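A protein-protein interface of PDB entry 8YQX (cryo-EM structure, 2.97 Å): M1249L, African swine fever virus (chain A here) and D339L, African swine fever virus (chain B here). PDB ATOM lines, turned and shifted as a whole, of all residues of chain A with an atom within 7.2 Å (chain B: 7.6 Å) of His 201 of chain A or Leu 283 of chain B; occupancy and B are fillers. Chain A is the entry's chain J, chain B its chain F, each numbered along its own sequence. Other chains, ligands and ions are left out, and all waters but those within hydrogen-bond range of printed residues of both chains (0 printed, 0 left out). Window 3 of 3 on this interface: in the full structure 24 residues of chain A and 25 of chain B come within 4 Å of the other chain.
The backbone carbonyl oxygen (O) of Leu 283 of chain B lies within hydrogen-bond range of a ring nitrogen (NE2) of His 201 of chain A.
NE2 of Gln 202 of chain A sits at hydrogen-bond distance from O of Ile 286 of chain B, 3.1 Å away.
CE1 of Phe 172 of chain A touches CG2 of Ile 285 of chain B (3.6 Å).
O of Ile 286 of chain B touches CD1 of Phe 172 of chain A, at 3.7 Å.
His 201 of chain A touches Pro 284 of chain B (CE1 to O, 3.5 Å).
CE1 of His 201 of chain A touches CA of Ile 285 of chain B (3.98 Å).
OE2 of Glu 205 of chain A touches CD1 of Ile 285 of chain B, 3.3 Å away.
The backbone carbonyl oxygen of Val 163 of chain B sits at hydrogen-bond distance from the backbone NH of Ile 285 of chain B, at 2.9 Å.
NE2 of Gln 202 of chain A sits at hydrogen-bond distance from O of Phe 172 of chain A, 2.7 Å away.
The side-chain amide oxygen (OE1) of Gln 202 of chain A lies within hydrogen-bond range of a ring nitrogen (ND1) of His 201 of chain A, at 3.3 Å.
Printed residues of chain A that touch a printed residue of chain B: Phe 172, His 201, Gln 202 and Glu 205.
Among the printed residues, no Asp or Glu carboxylate lies within 4 Å of a Lys or Arg side-chain nitrogen of the other chain.
Of the printed residues of chain B, His 201 of chain A touches Leu 283 (3.1 Å), Pro 284 (3.5 Å) and Ile 285 (3.98 Å).
Leu 283 of chain B touches just one residue of chain A: His 201.
Of the printed residues of chain B, Gln 202 of chain A touches Ile 286 (3.1 Å).
Of the printed residues of chain A, Pro 284 of chain B touches His 201.
Printed residues of chain A within 4 Å of Ile 285 of chain B: Phe 172 (3.6 Å), His 201 (3.98 Å) and Glu 205 (3.3 Å).
The nearest printed residue of chain B that does not touch His 201 of chain A is Ile 286 of chain B (5.2 Å).
The nearest residue of chain A that does not touch Leu 283 of chain B is Ile 197 of chain A (5.1 Å).
The nearest printed residue of chain A that does not touch Ile 286 of chain B is Gln 198 of chain A (4.8 Å).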
ATOM      1  N   ILE A  79      14.356 -11.396   1.665  1.00  0.00           N
ATOM      2  CA  ILE A  79      13.688 -11.238   2.952  1.00  0.00           C
ATOM      3  C   ILE A  79      12.601 -12.294   3.127  1.00  0.00           C
ATOM      4  O   ILE A  79      12.486 -12.915   4.192  1.00  0.00           O
ATOM      5  CB  ILE A  79      13.126  -9.811   3.087  1.00  0.00           C
ATOM      6  CG1 ILE A  79      14.267  -8.801   3.205  1.00  0.00           C
ATOM      7  CG2 ILE A  79      12.215  -9.708   4.295  1.00  0.00           C
ATOM      8  CD1 ILE A  79      13.813  -7.360   3.156  1.00  0.00           C
ATOM      9  N   LEU A  83      12.073 -15.371   5.708  1.00  0.00           N
ATOM     10  CA  LEU A  83      10.839 -15.530   6.473  1.00  0.00           C
ATOM     11  C   LEU A  83      10.176 -16.883   6.253  1.00  0.00           C
ATOM     12  O   LEU A  83       9.352 -17.294   7.077  1.00  0.00           O
ATOM     13  CB  LEU A  83       9.854 -14.417   6.116  1.00  0.00           C
ATOM     14  CG  LEU A  83       9.731 -13.263   7.112  1.00  0.00           C
ATOM     15  CD1 LEU A  83      10.995 -12.417   7.113  1.00  0.00           C
ATOM     16  CD2 LEU A  83       8.511 -12.413   6.801  1.00  0.00           C
ATOM     17  N   PHE A 172       2.626  -7.415  17.440  1.00  0.00           N
ATOM     18  CA  PHE A 172       3.470  -7.016  16.318  1.00  0.00           C
ATOM     19  C   PHE A 172       2.789  -7.290  14.984  1.00  0.00           C
ATOM     20  O   PHE A 172       3.063  -6.606  13.992  1.00  0.00           O
ATOM     21  CB  PHE A 172       4.813  -7.734  16.391  1.00  0.00           C
ATOM     22  CG  PHE A 172       5.837  -7.014  17.217  1.00  0.00           C
ATOM     23  CD1 PHE A 172       6.673  -6.072  16.644  1.00  0.00           C
ATOM     24  CD2 PHE A 172       5.960  -7.278  18.570  1.00  0.00           C
ATOM     25  CE1 PHE A 172       7.611  -5.407  17.407  1.00  0.00           C
ATOM     26  CE2 PHE A 172       6.896  -6.619  19.335  1.00  0.00           C
ATOM     27  CZ  PHE A 172       7.723  -5.683  18.754  1.00  0.00           C
ATOM     28  N   MET A 173       1.903  -8.284  14.946  1.00  0.00           N
ATOM     29  CA  MET A 173       1.099  -8.605  13.774  1.00  0.00           C
ATOM     30  C   MET A 173      -0.127  -7.699  13.716  1.00  0.00           C
ATOM     31  O   MET A 173      -0.135  -6.632  14.339  1.00  0.00           O
ATOM     32  CB  MET A 173       0.700 -10.080  13.782  1.00  0.00           C
ATOM     33  CG  MET A 173       1.877 -11.033  13.652  1.00  0.00           C
ATOM     34  SD  MET A 173       3.405 -10.233  13.123  1.00  0.00           S
ATOM     35  CE  MET A 173       3.191 -10.231  11.345  1.00  0.00           C
ATOM     36  N   GLU A 194       2.925  -3.600  -1.133  1.00  0.00           N
ATOM     37  CA  GLU A 194       3.540  -2.877  -0.022  1.00  0.00           C
ATOM     38  C   GLU A 194       3.232  -3.514   1.327  1.00  0.00           C
ATOM     39  O   GLU A 194       4.086  -3.510   2.223  1.00  0.00           O
ATOM     40  CB  GLU A 194       3.086  -1.418  -0.034  1.00  0.00           C
ATOM     41  CG  GLU A 194       3.637  -0.608  -1.195  1.00  0.00           C
ATOM     42  CD  GLU A 194       3.132   0.821  -1.201  1.00  0.00           C
ATOM     43  OE1 GLU A 194       2.218   1.134  -0.409  1.00  0.00           O
ATOM     44  OE2 GLU A 194       3.650   1.632  -1.997  1.00  0.00           O
ATOM     45  N   ASN A 195       2.025  -4.051   1.506  1.00  0.00           N
ATOM     46  CA  ASN A 195       1.693  -4.648   2.792  1.00  0.00           C
ATOM     47  C   ASN A 195       2.473  -5.930   3.051  1.00  0.00           C
ATOM     48  O   ASN A 195       2.628  -6.313   4.210  1.00  0.00           O
ATOM     49  CB  ASN A 195       0.191  -4.906   2.894  1.00  0.00           C
ATOM     50  CG  ASN A 195      -0.585  -3.667   3.293  1.00  0.00           C
ATOM     51  OD1 ASN A 195      -1.581  -3.315   2.661  1.00  0.00           O
ATOM     52  ND2 ASN A 195      -0.134  -3.002   4.349  1.00  0.00           N
ATOM     53  N   ILE A 196       2.987  -6.590   2.012  1.00  0.00           N
ATOM     54  CA  ILE A 196       3.921  -7.689   2.246  1.00  0.00           C
ATOM     55  C   ILE A 196       5.229  -7.157   2.822  1.00  0.00           C
ATOM     56  O   ILE A 196       5.837  -7.779   3.701  1.00  0.00           O
ATOM     57  CB  ILE A 196       4.145  -8.496   0.954  1.00  0.00           C
ATOM     58  CG1 ILE A 196       2.942  -9.397   0.675  1.00  0.00           C
ATOM     59  CG2 ILE A 196       5.413  -9.332   1.047  1.00  0.00           C
ATOM     60  CD1 ILE A 196       3.121 -10.301  -0.524  1.00  0.00           C
ATOM     61  N   ILE A 197       5.672  -5.989   2.350  1.00  0.00           N
ATOM     62  CA  ILE A 197       6.838  -5.345   2.947  1.00  0.00           C
ATOM     63  C   ILE A 197       6.561  -4.999   4.403  1.00  0.00           C
ATOM     64  O   ILE A 197       7.418  -5.184   5.277  1.00  0.00           O
ATOM     65  CB  ILE A 197       7.239  -4.101   2.132  1.00  0.00           C
ATOM     66  CG1 ILE A 197       7.576  -4.493   0.692  1.00  0.00           C
ATOM     67  CG2 ILE A 197       8.418  -3.394   2.780  1.00  0.00           C
ATOM     68  CD1 ILE A 197       7.987  -3.327  -0.176  1.00  0.00           C
ATOM     69  N   GLN A 198       5.359  -4.490   4.689  1.00  0.00           N
ATOM     70  CA  GLN A 198       4.993  -4.192   6.072  1.00  0.00           C
ATOM     71  C   GLN A 198       4.970  -5.457   6.925  1.00  0.00           C
ATOM     72  O   GLN A 198       5.409  -5.443   8.079  1.00  0.00           O
ATOM     73  CB  GLN A 198       3.636  -3.493   6.121  1.00  0.00           C
ATOM     74  CG  GLN A 198       3.326  -2.844   7.461  1.00  0.00           C
ATOM     75  CD  GLN A 198       1.900  -2.340   7.551  1.00  0.00           C
ATOM     76  OE1 GLN A 198       1.072  -2.628   6.687  1.00  0.00           O
ATOM     77  NE2 GLN A 198       1.607  -1.583   8.600  1.00  0.00           N
ATOM     78  N   PHE A 199       4.446  -6.554   6.374  1.00  0.00           N
ATOM     79  CA  PHE A 199       4.432  -7.829   7.084  1.00  0.00           C
ATOM     80  C   PHE A 199       5.844  -8.296   7.404  1.00  0.00           C
ATOM     81  O   PHE A 199       6.120  -8.747   8.522  1.00  0.00           O
ATOM     82  CB  PHE A 199       3.691  -8.871   6.243  1.00  0.00           C
ATOM     83  CG  PHE A 199       3.683 -10.255   6.832  1.00  0.00           C
ATOM     84  CD1 PHE A 199       4.748 -11.120   6.630  1.00  0.00           C
ATOM     85  CD2 PHE A 199       2.598 -10.702   7.565  1.00  0.00           C
ATOM     86  CE1 PHE A 199       4.740 -12.392   7.162  1.00  0.00           C
ATOM     87  CE2 PHE A 199       2.584 -11.976   8.098  1.00  0.00           C
ATOM     88  CZ  PHE A 199       3.657 -12.820   7.895  1.00  0.00           C
ATOM     89  N   THR A 200       6.749  -8.207   6.428  1.00  0.00           N
ATOM     90  CA  THR A 200       8.131  -8.613   6.663  1.00  0.00           C
ATOM     91  C   THR A 200       8.788  -7.736   7.719  1.00  0.00           C
ATOM     92  O   THR A 200       9.512  -8.234   8.591  1.00  0.00           O
ATOM     93  CB  THR A 200       8.923  -8.562   5.357  1.00  0.00           C
ATOM     94  OG1 THR A 200       8.766  -7.273   4.752  1.00  0.00           O
ATOM     95  CG2 THR A 200       8.431  -9.630   4.393  1.00  0.00           C
ATOM     96  N   HIS A 201       8.544  -6.424   7.659  1.00  0.00           N
ATOM     97  CA  HIS A 201       9.099  -5.517   8.659  1.00  0.00           C
ATOM     98  C   HIS A 201       8.584  -5.850  10.053  1.00  0.00           C
ATOM     99  O   HIS A 201       9.359  -5.887  11.017  1.00  0.00           O
ATOM    100  CB  HIS A 201       8.761  -4.072   8.289  1.00  0.00           C
ATOM    101  CG  HIS A 201       9.210  -3.065   9.300  1.00  0.00           C
ATOM    102  ND1 HIS A 201       8.370  -2.558  10.269  1.00  0.00           N
ATOM    103  CD2 HIS A 201      10.410  -2.466   9.493  1.00  0.00           C
ATOM    104  CE1 HIS A 201       9.033  -1.693  11.016  1.00  0.00           C
ATOM    105  NE2 HIS A 201      10.273  -1.619  10.564  1.00  0.00           N
ATOM    106  N   GLN A 202       7.279  -6.104  10.176  1.00  0.00           N
ATOM    107  CA  GLN A 202       6.707  -6.438  11.475  1.00  0.00           C
ATOM    108  C   GLN A 202       7.255  -7.758  12.000  1.00  0.00           C
ATOM    109  O   GLN A 202       7.539  -7.884  13.193  1.00  0.00           O
ATOM    110  CB  GLN A 202       5.182  -6.486  11.385  1.00  0.00           C
ATOM    111  CG  GLN A 202       4.531  -5.131  11.157  1.00  0.00           C
ATOM    112  CD  GLN A 202       4.895  -4.119  12.226  1.00  0.00           C
ATOM    113  OE1 GLN A 202       5.563  -3.124  11.952  1.00  0.00           O
ATOM    114  NE2 GLN A 202       4.455  -4.371  13.453  1.00  0.00           N
ATOM    115  N   TYR A 203       7.408  -8.756  11.126  1.00  0.00           N
ATOM    116  CA  TYR A 203       7.974 -10.034  11.548  1.00  0.00           C
ATOM    117  C   TYR A 203       9.411  -9.870  12.033  1.00  0.00           C
ATOM    118  O   TYR A 203       9.794 -10.416  13.080  1.00  0.00           O
ATOM    119  CB  TYR A 203       7.908 -11.031  10.390  1.00  0.00           C
ATOM    120  CG  TYR A 203       8.037 -12.482  10.790  1.00  0.00           C
ATOM    121  CD1 TYR A 203       6.938 -13.199  11.241  1.00  0.00           C
ATOM    122  CD2 TYR A 203       9.255 -13.140  10.702  1.00  0.00           C
ATOM    123  CE1 TYR A 203       7.051 -14.526  11.601  1.00  0.00           C
ATOM    124  CE2 TYR A 203       9.377 -14.468  11.059  1.00  0.00           C
ATOM    125  CZ  TYR A 203       8.272 -15.156  11.507  1.00  0.00           C
ATOM    126  OH  TYR A 203       8.391 -16.479  11.864  1.00  0.00           O
ATOM    127  N   ILE A 204      10.219  -9.112  11.286  1.00  0.00           N
ATOM    128  CA  ILE A 204      11.610  -8.898  11.673  1.00  0.00           C
ATOM    129  C   ILE A 204      11.683  -8.175  13.010  1.00  0.00           C
ATOM    130  O   ILE A 204      12.464  -8.552  13.893  1.00  0.00           O
ATOM    131  CB  ILE A 204      12.362  -8.130  10.571  1.00  0.00           C
ATOM    132  CG1 ILE A 204      12.521  -9.004   9.326  1.00  0.00           C
ATOM    133  CG2 ILE A 204      13.719  -7.662  11.072  1.00  0.00           C
ATOM    134  CD1 ILE A 204      13.243 -10.307   9.582  1.00  0.00           C
ATOM    135  N   GLU A 205      10.867  -7.134  13.186  1.00  0.00           N
ATOM    136  CA  GLU A 205      10.882  -6.395  14.444  1.00  0.00           C
ATOM    137  C   GLU A 205      10.385  -7.253  15.601  1.00  0.00           C
ATOM    138  O   GLU A 205      10.906  -7.159  16.717  1.00  0.00           O
ATOM    139  CB  GLU A 205      10.044  -5.125  14.312  1.00  0.00           C
ATOM    140  CG  GLU A 205      10.632  -4.090  13.365  1.00  0.00           C
ATOM    141  CD  GLU A 205      12.062  -3.716  13.709  1.00  0.00           C
ATOM    142  OE1 GLU A 205      12.843  -3.440  12.774  1.00  0.00           O
ATOM    143  OE2 GLU A 205      12.405  -3.684  14.910  1.00  0.00           O
ATOM    144  N   LEU A 206       9.383  -8.099  15.353  1.00  0.00           N
ATOM    145  CA  LEU A 206       8.880  -8.990  16.391  1.00  0.00           C
ATOM    146  C   LEU A 206       9.966  -9.946  16.860  1.00  0.00           C
ATOM    147  O   LEU A 206      10.151 -10.153  18.065  1.00  0.00           O
ATOM    148  CB  LEU A 206       7.673  -9.769  15.868  1.00  0.00           C
ATOM    149  CG  LEU A 206       7.312 -11.057  16.610  1.00  0.00           C
ATOM    150  CD1 LEU A 206       6.712 -10.746  17.970  1.00  0.00           C
ATOM    151  CD2 LEU A 206       6.362 -11.904  15.781  1.00  0.00           C
ATOM    152  N   TYR A 207      10.705 -10.535  15.921  1.00  0.00           N
ATOM    153  CA  TYR A 207      11.739 -11.476  16.338  1.00  0.00           C
ATOM    154  C   TYR A 207      12.937 -10.762  16.954  1.00  0.00           C
ATOM    155  O   TYR A 207      13.589 -11.313  17.849  1.00  0.00           O
ATOM    156  CB  TYR A 207      12.154 -12.364  15.169  1.00  0.00           C
ATOM    157  CG  TYR A 207      11.379 -13.662  15.145  1.00  0.00           C
ATOM    158  CD1 TYR A 207       9.992 -13.661  15.207  1.00  0.00           C
ATOM    159  CD2 TYR A 207      12.030 -14.886  15.093  1.00  0.00           C
ATOM    160  CE1 TYR A 207       9.275 -14.840  15.198  1.00  0.00           C
ATOM    161  CE2 TYR A 207      11.320 -16.073  15.083  1.00  0.00           C
ATOM    162  CZ  TYR A 207       9.941 -16.042  15.136  1.00  0.00           C
ATOM    163  OH  TYR A 207       9.226 -17.218  15.127  1.00  0.00           O
ATOM    164  N   SER B 162      15.299   4.090  16.877  1.00  0.00           N
ATOM    165  CA  SER B 162      14.074   3.446  16.429  1.00  0.00           C
ATOM    166  C   SER B 162      12.872   4.189  16.991  1.00  0.00           C
ATOM    167  O   SER B 162      12.908   4.708  18.108  1.00  0.00           O
ATOM    168  CB  SER B 162      14.025   1.974  16.856  1.00  0.00           C
ATOM    169  OG  SER B 162      15.076   1.234  16.258  1.00  0.00           O
ATOM    170  N   VAL B 163      11.803   4.233  16.200  1.00  0.00           N
ATOM    171  CA  VAL B 163      10.556   4.888  16.576  1.00  0.00           C
ATOM    172  C   VAL B 163       9.486   3.817  16.724  1.00  0.00           C
ATOM    173  O   VAL B 163       9.324   2.969  15.841  1.00  0.00           O
ATOM    174  CB  VAL B 163      10.137   5.945  15.539  1.00  0.00           C
ATOM    175  CG1 VAL B 163       8.767   6.508  15.880  1.00  0.00           C
ATOM    176  CG2 VAL B 163      11.169   7.055  15.468  1.00  0.00           C
ATOM    177  N   TYR B 164       8.766   3.850  17.841  1.00  0.00           N
ATOM    178  CA  TYR B 164       7.734   2.870  18.145  1.00  0.00           C
ATOM    179  C   TYR B 164       6.369   3.540  18.065  1.00  0.00           C
ATOM    180  O   TYR B 164       6.096   4.488  18.807  1.00  0.00           O
ATOM    181  CB  TYR B 164       7.952   2.260  19.530  1.00  0.00           C
ATOM    182  CG  TYR B 164       9.217   1.439  19.650  1.00  0.00           C
ATOM    183  CD1 TYR B 164       9.207   0.074  19.407  1.00  0.00           C
ATOM    184  CD2 TYR B 164      10.419   2.030  20.016  1.00  0.00           C
ATOM    185  CE1 TYR B 164      10.358  -0.679  19.517  1.00  0.00           C
ATOM    186  CE2 TYR B 164      11.575   1.286  20.127  1.00  0.00           C
ATOM    187  CZ  TYR B 164      11.539  -0.068  19.877  1.00  0.00           C
ATOM    188  OH  TYR B 164      12.687  -0.817  19.987  1.00  0.00           O
ATOM    189  N   ASN B 276       4.480  11.353  13.635  1.00  0.00           N
ATOM    190  CA  ASN B 276       5.839  10.849  13.437  1.00  0.00           C
ATOM    191  C   ASN B 276       6.719  11.999  12.956  1.00  0.00           C
ATOM    192  O   ASN B 276       7.030  12.143  11.770  1.00  0.00           O
ATOM    193  CB  ASN B 276       5.843   9.687  12.454  1.00  0.00           C
ATOM    194  CG  ASN B 276       7.173   8.962  12.414  1.00  0.00           C
ATOM    195  OD1 ASN B 276       8.055   9.214  13.233  1.00  0.00           O
ATOM    196  ND2 ASN B 276       7.322   8.053  11.459  1.00  0.00           N
ATOM    197  N   ALA B 280      13.574   9.590  11.461  1.00  0.00           N
ATOM    198  CA  ALA B 280      14.156   8.258  11.437  1.00  0.00           C
ATOM    199  C   ALA B 280      14.301   7.763  10.000  1.00  0.00           C
ATOM    200  O   ALA B 280      13.609   8.214   9.083  1.00  0.00           O
ATOM    201  CB  ALA B 280      13.299   7.289  12.249  1.00  0.00           C
ATOM    202  N   THR B 281      15.219   6.816   9.811  1.00  0.00           N
ATOM    203  CA  THR B 281      15.539   6.285   8.490  1.00  0.00           C
ATOM    204  C   THR B 281      15.001   4.871   8.289  1.00  0.00           C
ATOM    205  O   THR B 281      15.557   4.095   7.507  1.00  0.00           O
ATOM    206  CB  THR B 281      17.048   6.314   8.255  1.00  0.00           C
ATOM    207  OG1 THR B 281      17.683   5.340   9.092  1.00  0.00           O
ATOM    208  CG2 THR B 281      17.606   7.689   8.580  1.00  0.00           C
ATOM    209  N   GLU B 282      13.922   4.520   8.985  1.00  0.00           N
ATOM    210  CA  GLU B 282      13.299   3.215   8.811  1.00  0.00           C
ATOM    211  C   GLU B 282      11.822   3.334   9.156  1.00  0.00           C
ATOM    212  O   GLU B 282      11.375   4.325   9.739  1.00  0.00           O
ATOM    213  CB  GLU B 282      13.976   2.136   9.671  1.00  0.00           C
ATOM    214  CG  GLU B 282      13.768   2.200  11.206  1.00  0.00           C
ATOM    215  CD  GLU B 282      13.953   3.568  11.866  1.00  0.00           C
ATOM    216  OE1 GLU B 282      14.393   4.537  11.211  1.00  0.00           O
ATOM    217  OE2 GLU B 282      13.656   3.669  13.073  1.00  0.00           O
ATOM    218  N   LEU B 283      11.068   2.308   8.781  1.00  0.00           N
ATOM    219  CA  LEU B 283       9.640   2.288   9.071  1.00  0.00           C
ATOM    220  C   LEU B 283       9.418   2.196  10.576  1.00  0.00           C
ATOM    221  O   LEU B 283      10.053   1.369  11.240  1.00  0.00           O
ATOM    222  CB  LEU B 283       8.968   1.111   8.367  1.00  0.00           C
ATOM    223  CG  LEU B 283       8.176   1.413   7.094  1.00  0.00           C
ATOM    224  CD1 LEU B 283       8.946   2.356   6.187  1.00  0.00           C
ATOM    225  CD2 LEU B 283       7.847   0.122   6.366  1.00  0.00           C
ATOM    226  N   PRO B 284       8.553   3.030  11.152  1.00  0.00           N
ATOM    227  CA  PRO B 284       8.252   2.908  12.582  1.00  0.00           C
ATOM    228  C   PRO B 284       7.726   1.520  12.919  1.00  0.00           C
ATOM    229  O   PRO B 284       6.965   0.919  12.158  1.00  0.00           O
ATOM    230  CB  PRO B 284       7.185   3.985  12.820  1.00  0.00           C
ATOM    231  CG  PRO B 284       6.997   4.705  11.512  1.00  0.00           C
ATOM    232  CD  PRO B 284       8.111   4.321  10.604  1.00  0.00           C
ATOM    233  N   ILE B 285       8.142   1.017  14.074  1.00  0.00           N
ATOM    234  CA  ILE B 285       7.771  -0.316  14.532  1.00  0.00           C
ATOM    235  C   ILE B 285       6.418  -0.233  15.225  1.00  0.00           C
ATOM    236  O   ILE B 285       6.275   0.457  16.237  1.00  0.00           O
ATOM    237  CB  ILE B 285       8.835  -0.886  15.480  1.00  0.00           C
ATOM    238  CG1 ILE B 285      10.222  -0.795  14.841  1.00  0.00           C
ATOM    239  CG2 ILE B 285       8.492  -2.311  15.867  1.00  0.00           C
ATOM    240  CD1 ILE B 285      11.351  -0.729  15.842  1.00  0.00           C
ATOM    241  N   ILE B 286       5.427  -0.938  14.690  1.00  0.00           N
ATOM    242  CA  ILE B 286       4.111  -0.986  15.316  1.00  0.00           C
ATOM    243  C   ILE B 286       4.182  -1.941  16.499  1.00  0.00           C
ATOM    244  O   ILE B 286       4.473  -3.130  16.332  1.00  0.00           O
ATOM    245  CB  ILE B 286       3.033  -1.424  14.315  1.00  0.00           C
ATOM    246  CG1 ILE B 286       3.118  -0.591  13.034  1.00  0.00           C
ATOM    247  CG2 ILE B 286       1.651  -1.307  14.938  1.00  0.00           C
ATOM    248  CD1 ILE B 286       2.796   0.867  13.230  1.00  0.00           C
